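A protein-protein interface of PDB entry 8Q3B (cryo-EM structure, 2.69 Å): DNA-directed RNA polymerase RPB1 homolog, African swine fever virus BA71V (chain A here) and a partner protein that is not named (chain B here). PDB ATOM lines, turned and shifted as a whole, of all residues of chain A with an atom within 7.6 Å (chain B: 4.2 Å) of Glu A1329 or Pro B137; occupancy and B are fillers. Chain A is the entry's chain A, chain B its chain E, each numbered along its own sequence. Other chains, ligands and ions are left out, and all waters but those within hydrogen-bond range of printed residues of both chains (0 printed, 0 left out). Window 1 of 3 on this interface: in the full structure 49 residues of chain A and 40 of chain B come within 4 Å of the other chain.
The guanidinium group of Arg B186 lies within salt-bridge range of the side-chain carboxylate of Glu A1329, 2.7 Å away. OE2 of Glu A1329 is in salt-bridge range of NH1 of Arg B198, at 2.8 Å. NH1 of Arg B186 lies within salt-bridge range of OD1 of Asp A1358, at 3.3 Å. NH2 of Arg B198 sits at hydrogen-bond distance from O of Thr A1361, 2.9 Å away.
Of chain B, only Pro B137 (3.5 Å), His B139 (3.7 Å), Ile B184 (3.7 Å), Arg B186 (2.7 Å) and Arg B198 (2.8 Å) come within 4 Å of Glu A1329. Lys A1334 touches none of the printed residues of chain B. Of the printed residues of chain B, Thr A1361 touches Arg B198 (2.9 Å). Pro B137 touches just one residue of chain A: Glu A1329. Of the printed residues of chain A, Arg B198 touches Glu A1329, Thr A1361 and Gly A1364. The nearest printed residue of chain B that does not touch Glu A1329 is Ala B135 (5.0 Å). The nearest printed residue of chain B that does not touch Tyr A1326 is Ala B135 (4.2 Å).
Of the 18 printed residues of chain A, 8 touch a printed residue of chain B. Printed residues of chain A that touch a printed residue of chain B: Phe A918, Tyr A1326, Glu A1329, Ala A1330, Arg A1332, Asp A1358, Thr A1361 and Gly A1364. Of the 9 printed residues of chain B, 7 touch a printed residue of chain A. Among the printed residues, Asp or Glu carboxylates within 4 Å of a Lys or Arg side-chain nitrogen of the other chain: Glu A1329 with Arg B186 (2.7 Å), Glu A1329 with Arg B198 (2.8 Å) and Asp A1358 with Arg B186 (3.3 Å).
The guanidinium group (NH1) of Arg A1332 lies within salt-bridge range of the side-chain carboxylate (OD2) of Asp A1358, 2.7 Å away. The backbone carbonyl oxygen of Pro B137 sits at hydrogen-bond distance from a ring nitrogen (ND1) of His B139 (3.0 Å).
Among the printed residues, merely in contact across the chains: Phe A918 with Ala B135, Tyr A1326 with Ile B136, Glu A1329 with Pro B137, Glu A1329 with His B139, Glu A1329 with Ile B184, Ala A1330 with Ala B135, Arg A1332 with Arg B186 and Gly A1364 with Arg B198.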
ATOM      1  N   ASN A 914     -14.180  30.526  15.385  1.00  0.00           N
ATOM      2  CA  ASN A 914     -15.129  29.519  15.846  1.00  0.00           C
ATOM      3  C   ASN A 914     -15.107  28.295  14.941  1.00  0.00           C
ATOM      4  O   ASN A 914     -15.200  27.159  15.416  1.00  0.00           O
ATOM      5  CB  ASN A 914     -16.534  30.115  15.909  1.00  0.00           C
ATOM      6  CG  ASN A 914     -17.554  29.140  16.452  1.00  0.00           C
ATOM      7  OD1 ASN A 914     -18.083  28.305  15.719  1.00  0.00           O
ATOM      8  ND2 ASN A 914     -17.834  29.236  17.746  1.00  0.00           N
ATOM      9  N   PHE A 918     -14.005  23.988  16.129  1.00  0.00           N
ATOM     10  CA  PHE A 918     -14.698  22.705  16.079  1.00  0.00           C
ATOM     11  C   PHE A 918     -14.163  21.797  14.976  1.00  0.00           C
ATOM     12  O   PHE A 918     -14.860  20.873  14.544  1.00  0.00           O
ATOM     13  CB  PHE A 918     -16.216  22.902  15.951  1.00  0.00           C
ATOM     14  CG  PHE A 918     -16.672  23.589  14.683  1.00  0.00           C
ATOM     15  CD1 PHE A 918     -16.523  22.994  13.440  1.00  0.00           C
ATOM     16  CD2 PHE A 918     -17.306  24.818  14.751  1.00  0.00           C
ATOM     17  CE1 PHE A 918     -16.964  23.627  12.294  1.00  0.00           C
ATOM     18  CE2 PHE A 918     -17.753  25.450  13.609  1.00  0.00           C
ATOM     19  CZ  PHE A 918     -17.579  24.854  12.381  1.00  0.00           C
ATOM     20  N   THR A1322     -21.321  13.137  18.268  1.00  0.00           N
ATOM     21  CA  THR A1322     -21.631  14.555  18.117  1.00  0.00           C
ATOM     22  C   THR A1322     -23.134  14.776  18.012  1.00  0.00           C
ATOM     23  O   THR A1322     -23.678  15.703  18.623  1.00  0.00           O
ATOM     24  CB  THR A1322     -20.923  15.118  16.887  1.00  0.00           C
ATOM     25  OG1 THR A1322     -19.565  14.664  16.864  1.00  0.00           O
ATOM     26  CG2 THR A1322     -20.942  16.637  16.908  1.00  0.00           C
ATOM     27  N   MET A1323     -23.823  13.935  17.238  1.00  0.00           N
ATOM     28  CA  MET A1323     -25.272  14.055  17.125  1.00  0.00           C
ATOM     29  C   MET A1323     -25.943  13.824  18.473  1.00  0.00           C
ATOM     30  O   MET A1323     -26.881  14.541  18.840  1.00  0.00           O
ATOM     31  CB  MET A1323     -25.793  13.064  16.083  1.00  0.00           C
ATOM     32  CG  MET A1323     -27.308  12.897  16.048  1.00  0.00           C
ATOM     33  SD  MET A1323     -28.166  14.363  15.448  1.00  0.00           S
ATOM     34  CE  MET A1323     -29.859  13.942  15.844  1.00  0.00           C
ATOM     35  N   TYR A1326     -24.545  16.952  21.052  1.00  0.00           N
ATOM     36  CA  TYR A1326     -24.679  18.354  20.667  1.00  0.00           C
ATOM     37  C   TYR A1326     -25.980  18.638  19.923  1.00  0.00           C
ATOM     38  O   TYR A1326     -26.767  19.483  20.358  1.00  0.00           O
ATOM     39  CB  TYR A1326     -23.468  18.769  19.820  1.00  0.00           C
ATOM     40  CG  TYR A1326     -22.159  18.793  20.589  1.00  0.00           C
ATOM     41  CD1 TYR A1326     -22.137  18.943  21.970  1.00  0.00           C
ATOM     42  CD2 TYR A1326     -20.946  18.660  19.930  1.00  0.00           C
ATOM     43  CE1 TYR A1326     -20.949  18.964  22.669  1.00  0.00           C
ATOM     44  CE2 TYR A1326     -19.752  18.679  20.623  1.00  0.00           C
ATOM     45  CZ  TYR A1326     -19.760  18.831  21.991  1.00  0.00           C
ATOM     46  OH  TYR A1326     -18.574  18.851  22.686  1.00  0.00           O
ATOM     47  N   GLY A1327     -26.223  17.961  18.813  1.00  0.00           N
ATOM     48  CA  GLY A1327     -27.462  18.140  18.086  1.00  0.00           C
ATOM     49  C   GLY A1327     -27.265  17.907  16.602  1.00  0.00           C
ATOM     50  O   GLY A1327     -26.216  17.457  16.155  1.00  0.00           O
ATOM     51  N   ILE A1328     -28.318  18.228  15.846  1.00  0.00           N
ATOM     52  CA  ILE A1328     -28.319  17.957  14.412  1.00  0.00           C
ATOM     53  C   ILE A1328     -27.375  18.900  13.676  1.00  0.00           C
ATOM     54  O   ILE A1328     -26.712  18.502  12.713  1.00  0.00           O
ATOM     55  CB  ILE A1328     -29.753  18.038  13.856  1.00  0.00           C
ATOM     56  CG1 ILE A1328     -29.797  17.539  12.410  1.00  0.00           C
ATOM     57  CG2 ILE A1328     -30.286  19.459  13.938  1.00  0.00           C
ATOM     58  CD1 ILE A1328     -29.398  16.088  12.247  1.00  0.00           C
ATOM     59  N   GLU A1329     -27.313  20.167  14.091  1.00  0.00           N
ATOM     60  CA  GLU A1329     -26.423  21.113  13.421  1.00  0.00           C
ATOM     61  C   GLU A1329     -24.960  20.744  13.638  1.00  0.00           C
ATOM     62  O   GLU A1329     -24.150  20.792  12.701  1.00  0.00           O
ATOM     63  CB  GLU A1329     -26.699  22.529  13.919  1.00  0.00           C
ATOM     64  CG  GLU A1329     -28.115  23.012  13.658  1.00  0.00           C
ATOM     65  CD  GLU A1329     -28.422  23.153  12.182  1.00  0.00           C
ATOM     66  OE1 GLU A1329     -27.752  23.963  11.510  1.00  0.00           O
ATOM     67  OE2 GLU A1329     -29.333  22.455  11.693  1.00  0.00           O
ATOM     68  N   ALA A1330     -24.601  20.379  14.871  1.00  0.00           N
ATOM     69  CA  ALA A1330     -23.249  19.900  15.128  1.00  0.00           C
ATOM     70  C   ALA A1330     -22.967  18.636  14.330  1.00  0.00           C
ATOM     71  O   ALA A1330     -21.850  18.439  13.841  1.00  0.00           O
ATOM     72  CB  ALA A1330     -23.058  19.647  16.622  1.00  0.00           C
ATOM     73  N   ALA A1331     -23.971  17.769  14.184  1.00  0.00           N
ATOM     74  CA  ALA A1331     -23.799  16.572  13.370  1.00  0.00           C
ATOM     75  C   ALA A1331     -23.528  16.932  11.915  1.00  0.00           C
ATOM     76  O   ALA A1331     -22.691  16.304  11.260  1.00  0.00           O
ATOM     77  CB  ALA A1331     -25.038  15.686  13.479  1.00  0.00           C
ATOM     78  N   ARG A1332     -24.233  17.934  11.389  1.00  0.00           N
ATOM     79  CA  ARG A1332     -24.009  18.366  10.012  1.00  0.00           C
ATOM     80  C   ARG A1332     -22.597  18.907   9.834  1.00  0.00           C
ATOM     81  O   ARG A1332     -21.903  18.576   8.860  1.00  0.00           O
ATOM     82  CB  ARG A1332     -25.046  19.426   9.639  1.00  0.00           C
ATOM     83  CG  ARG A1332     -25.086  19.784   8.168  1.00  0.00           C
ATOM     84  CD  ARG A1332     -25.876  21.059   7.942  1.00  0.00           C
ATOM     85  NE  ARG A1332     -25.025  22.242   7.961  1.00  0.00           N
ATOM     86  CZ  ARG A1332     -24.623  22.907   6.885  1.00  0.00           C
ATOM     87  NH1 ARG A1332     -24.966  22.527   5.665  1.00  0.00           N
ATOM     88  NH2 ARG A1332     -23.855  23.981   7.037  1.00  0.00           N
ATOM     89  N   GLN A1333     -22.150  19.742  10.773  1.00  0.00           N
ATOM     90  CA  GLN A1333     -20.793  20.273  10.690  1.00  0.00           C
ATOM     91  C   GLN A1333     -19.766  19.150  10.772  1.00  0.00           C
ATOM     92  O   GLN A1333     -18.760  19.162  10.050  1.00  0.00           O
ATOM     93  CB  GLN A1333     -20.562  21.298  11.799  1.00  0.00           C
ATOM     94  CG  GLN A1333     -21.384  22.566  11.644  1.00  0.00           C
ATOM     95  CD  GLN A1333     -20.903  23.440  10.505  1.00  0.00           C
ATOM     96  OE1 GLN A1333     -19.961  23.091   9.795  1.00  0.00           O
ATOM     97  NE2 GLN A1333     -21.549  24.585  10.323  1.00  0.00           N
ATOM     98  N   LYS A1334     -20.003  18.169  11.644  1.00  0.00           N
ATOM     99  CA  LYS A1334     -19.086  17.042  11.757  1.00  0.00           C
ATOM    100  C   LYS A1334     -19.065  16.219  10.477  1.00  0.00           C
ATOM    101  O   LYS A1334     -18.010  15.723  10.071  1.00  0.00           O
ATOM    102  CB  LYS A1334     -19.474  16.168  12.948  1.00  0.00           C
ATOM    103  CG  LYS A1334     -18.418  15.146  13.348  1.00  0.00           C
ATOM    104  CD  LYS A1334     -17.082  15.789  13.699  1.00  0.00           C
ATOM    105  CE  LYS A1334     -17.213  16.780  14.842  1.00  0.00           C
ATOM    106  NZ  LYS A1334     -15.889  17.264  15.311  1.00  0.00           N
ATOM    107  N   ILE A1335     -20.221  16.042   9.839  1.00  0.00           N
ATOM    108  CA  ILE A1335     -20.261  15.327   8.567  1.00  0.00           C
ATOM    109  C   ILE A1335     -19.410  16.057   7.538  1.00  0.00           C
ATOM    110  O   ILE A1335     -18.616  15.445   6.813  1.00  0.00           O
ATOM    111  CB  ILE A1335     -21.714  15.168   8.085  1.00  0.00           C
ATOM    112  CG1 ILE A1335     -22.465  14.178   8.977  1.00  0.00           C
ATOM    113  CG2 ILE A1335     -21.747  14.701   6.635  1.00  0.00           C
ATOM    114  CD1 ILE A1335     -23.965  14.176   8.767  1.00  0.00           C
ATOM    115  N   ILE A1336     -19.560  17.380   7.466  1.00  0.00           N
ATOM    116  CA  ILE A1336     -18.756  18.158   6.525  1.00  0.00           C
ATOM    117  C   ILE A1336     -17.273  17.950   6.809  1.00  0.00           C
ATOM    118  O   ILE A1336     -16.479  17.680   5.900  1.00  0.00           O
ATOM    119  CB  ILE A1336     -19.133  19.649   6.595  1.00  0.00           C
ATOM    120  CG1 ILE A1336     -20.504  19.883   5.966  1.00  0.00           C
ATOM    121  CG2 ILE A1336     -18.093  20.496   5.883  1.00  0.00           C
ATOM    122  CD1 ILE A1336     -21.283  21.003   6.610  1.00  0.00           C
ATOM    123  N   ASP A1358     -26.240  18.410   4.146  1.00  0.00           N
ATOM    124  CA  ASP A1358     -27.618  18.881   4.217  1.00  0.00           C
ATOM    125  C   ASP A1358     -28.598  17.776   3.851  1.00  0.00           C
ATOM    126  O   ASP A1358     -29.625  17.608   4.516  1.00  0.00           O
ATOM    127  CB  ASP A1358     -27.803  20.085   3.295  1.00  0.00           C
ATOM    128  CG  ASP A1358     -27.367  21.383   3.940  1.00  0.00           C
ATOM    129  OD1 ASP A1358     -27.941  21.753   4.985  1.00  0.00           O
ATOM    130  OD2 ASP A1358     -26.448  22.035   3.403  1.00  0.00           O
ATOM    131  N   THR A1361     -29.036  15.085   6.600  1.00  0.00           N
ATOM    132  CA  THR A1361     -29.528  15.538   7.898  1.00  0.00           C
ATOM    133  C   THR A1361     -30.767  16.420   7.778  1.00  0.00           C
ATOM    134  O   THR A1361     -31.041  17.213   8.685  1.00  0.00           O
ATOM    135  CB  THR A1361     -28.431  16.296   8.648  1.00  0.00           C
ATOM    136  OG1 THR A1361     -27.966  17.385   7.844  1.00  0.00           O
ATOM    137  CG2 THR A1361     -27.266  15.376   8.963  1.00  0.00           C
ATOM    138  N   GLY A1364     -33.922  15.866  10.492  1.00  0.00           N
ATOM    139  CA  GLY A1364     -33.665  15.995  11.907  1.00  0.00           C
ATOM    140  C   GLY A1364     -32.821  14.888  12.495  1.00  0.00           C
ATOM    141  O   GLY A1364     -32.441  14.978  13.670  1.00  0.00           O
ATOM    142  N   ALA B 135     -19.295  24.285  18.956  1.00  0.00           N
ATOM    143  CA  ALA B 135     -19.759  23.513  17.809  1.00  0.00           C
ATOM    144  C   ALA B 135     -21.247  23.680  17.536  1.00  0.00           C
ATOM    145  O   ALA B 135     -21.706  23.281  16.460  1.00  0.00           O
ATOM    146  CB  ALA B 135     -19.443  22.032  18.016  1.00  0.00           C
ATOM    147  N   ILE B 136     -22.005  24.250  18.463  1.00  0.00           N
ATOM    148  CA  ILE B 136     -23.454  24.383  18.334  1.00  0.00           C
ATOM    149  C   ILE B 136     -23.754  25.781  17.802  1.00  0.00           C
ATOM    150  O   ILE B 136     -23.450  26.767  18.490  1.00  0.00           O
ATOM    151  CB  ILE B 136     -24.158  24.139  19.677  1.00  0.00           C
ATOM    152  CG1 ILE B 136     -23.992  22.675  20.087  1.00  0.00           C
ATOM    153  CG2 ILE B 136     -25.635  24.510  19.584  1.00  0.00           C
ATOM    154  CD1 ILE B 136     -24.564  22.339  21.440  1.00  0.00           C
ATOM    155  N   PRO B 137     -24.344  25.917  16.604  1.00  0.00           N
ATOM    156  CA  PRO B 137     -24.691  27.258  16.111  1.00  0.00           C
ATOM    157  C   PRO B 137     -25.700  27.955  17.008  1.00  0.00           C
ATOM    158  O   PRO B 137     -26.197  27.363  17.970  1.00  0.00           O
ATOM    159  CB  PRO B 137     -25.274  26.988  14.717  1.00  0.00           C
ATOM    160  CG  PRO B 137     -24.815  25.631  14.350  1.00  0.00           C
ATOM    161  CD  PRO B 137     -24.675  24.872  15.624  1.00  0.00           C
ATOM    162  N   LYS B 138     -26.009  29.211  16.703  1.00  0.00           N
ATOM    163  CA  LYS B 138     -26.935  29.996  17.509  1.00  0.00           C
ATOM    164  C   LYS B 138     -28.363  29.714  17.060  1.00  0.00           C
ATOM    165  O   LYS B 138     -28.737  30.024  15.922  1.00  0.00           O
ATOM    166  CB  LYS B 138     -26.620  31.487  17.397  1.00  0.00           C
ATOM    167  CG  LYS B 138     -26.053  32.108  18.668  1.00  0.00           C
ATOM    168  CD  LYS B 138     -24.874  31.317  19.217  1.00  0.00           C
ATOM    169  CE  LYS B 138     -24.203  32.044  20.369  1.00  0.00           C
ATOM    170  NZ  LYS B 138     -23.763  31.100  21.432  1.00  0.00           N
ATOM    171  N   HIS B 139     -29.153  29.126  17.954  1.00  0.00           N
ATOM    172  CA  HIS B 139     -30.561  28.855  17.717  1.00  0.00           C
ATOM    173  C   HIS B 139     -31.417  29.940  18.358  1.00  0.00           C
ATOM    174  O   HIS B 139     -31.017  30.577  19.335  1.00  0.00           O
ATOM    175  CB  HIS B 139     -30.962  27.490  18.284  1.00  0.00           C
ATOM    176  CG  HIS B 139     -30.296  26.331  17.611  1.00  0.00           C
ATOM    177  ND1 HIS B 139     -28.929  26.230  17.477  1.00  0.00           N
ATOM    178  CD2 HIS B 139     -30.812  25.216  17.044  1.00  0.00           C
ATOM    179  CE1 HIS B 139     -28.631  25.106  16.850  1.00  0.00           C
ATOM    180  NE2 HIS B 139     -29.757  24.472  16.577  1.00  0.00           N
ATOM    181  N   ILE B 184     -31.759  29.273  12.841  1.00  0.00           N
ATOM    182  CA  ILE B 184     -30.392  28.898  13.173  1.00  0.00           C
ATOM    183  C   ILE B 184     -29.450  29.765  12.353  1.00  0.00           C
ATOM    184  O   ILE B 184     -29.598  29.866  11.127  1.00  0.00           O
ATOM    185  CB  ILE B 184     -30.130  27.405  12.905  1.00  0.00           C
ATOM    186  CG1 ILE B 184     -31.106  26.537  13.700  1.00  0.00           C
ATOM    187  CG2 ILE B 184     -28.701  27.040  13.266  1.00  0.00           C
ATOM    188  CD1 ILE B 184     -31.655  25.370  12.918  1.00  0.00           C
ATOM    189  N   GLU B 185     -28.489  30.391  13.033  1.00  0.00           N
ATOM    190  CA  GLU B 185     -27.476  31.233  12.398  1.00  0.00           C
ATOM    191  C   GLU B 185     -26.213  30.392  12.240  1.00  0.00           C
ATOM    192  O   GLU B 185     -25.352  30.352  13.118  1.00  0.00           O
ATOM    193  CB  GLU B 185     -27.220  32.490  13.221  1.00  0.00           C
ATOM    194  CG  GLU B 185     -27.854  33.747  12.647  1.00  0.00           C
ATOM    195  CD  GLU B 185     -27.020  34.379  11.548  1.00  0.00           C
ATOM    196  OE1 GLU B 185     -25.972  33.804  11.187  1.00  0.00           O
ATOM    197  OE2 GLU B 185     -27.412  35.453  11.047  1.00  0.00           O
ATOM    198  N   ARG B 186     -26.110  29.721  11.107  1.00  0.00           N
ATOM    199  CA  ARG B 186     -24.984  28.838  10.851  1.00  0.00           C
ATOM    200  C   ARG B 186     -23.745  29.641  10.458  1.00  0.00           C
ATOM    201  O   ARG B 186     -23.854  30.650   9.752  1.00  0.00           O
ATOM    202  CB  ARG B 186     -25.313  27.851   9.735  1.00  0.00           C
ATOM    203  CG  ARG B 186     -26.513  26.964   9.995  1.00  0.00           C
ATOM    204  CD  ARG B 186     -26.910  26.221   8.732  1.00  0.00           C
ATOM    205  NE  ARG B 186     -27.734  25.052   9.012  1.00  0.00           N
ATOM    206  CZ  ARG B 186     -28.229  24.247   8.083  1.00  0.00           C
ATOM    207  NH1 ARG B 186     -27.998  24.451   6.797  1.00  0.00           N
ATOM    208  NH2 ARG B 186     -28.971  23.206   8.453  1.00  0.00           N
ATOM    209  N   ARG B 198     -36.036  25.944  10.712  1.00  0.00           N
ATOM    210  CA  ARG B 198     -36.365  24.537  10.857  1.00  0.00           C
ATOM    211  C   ARG B 198     -37.654  24.380  11.650  1.00  0.00           C
ATOM    212  O   ARG B 198     -37.944  25.156  12.568  1.00  0.00           O
ATOM    213  CB  ARG B 198     -35.230  23.774  11.547  1.00  0.00           C
ATOM    214  CG  ARG B 198     -33.957  23.699  10.722  1.00  0.00           C
ATOM    215  CD  ARG B 198     -32.909  22.822  11.382  1.00  0.00           C
ATOM    216  NE  ARG B 198     -33.051  21.421  10.998  1.00  0.00           N
ATOM    217  CZ  ARG B 198     -32.177  20.734  10.274  1.00  0.00           C
ATOM    218  NH1 ARG B 198     -31.067  21.287   9.809  1.00  0.00           N
ATOM    219  NH2 ARG B 198     -32.422  19.456  10.005  1.00  0.00           N
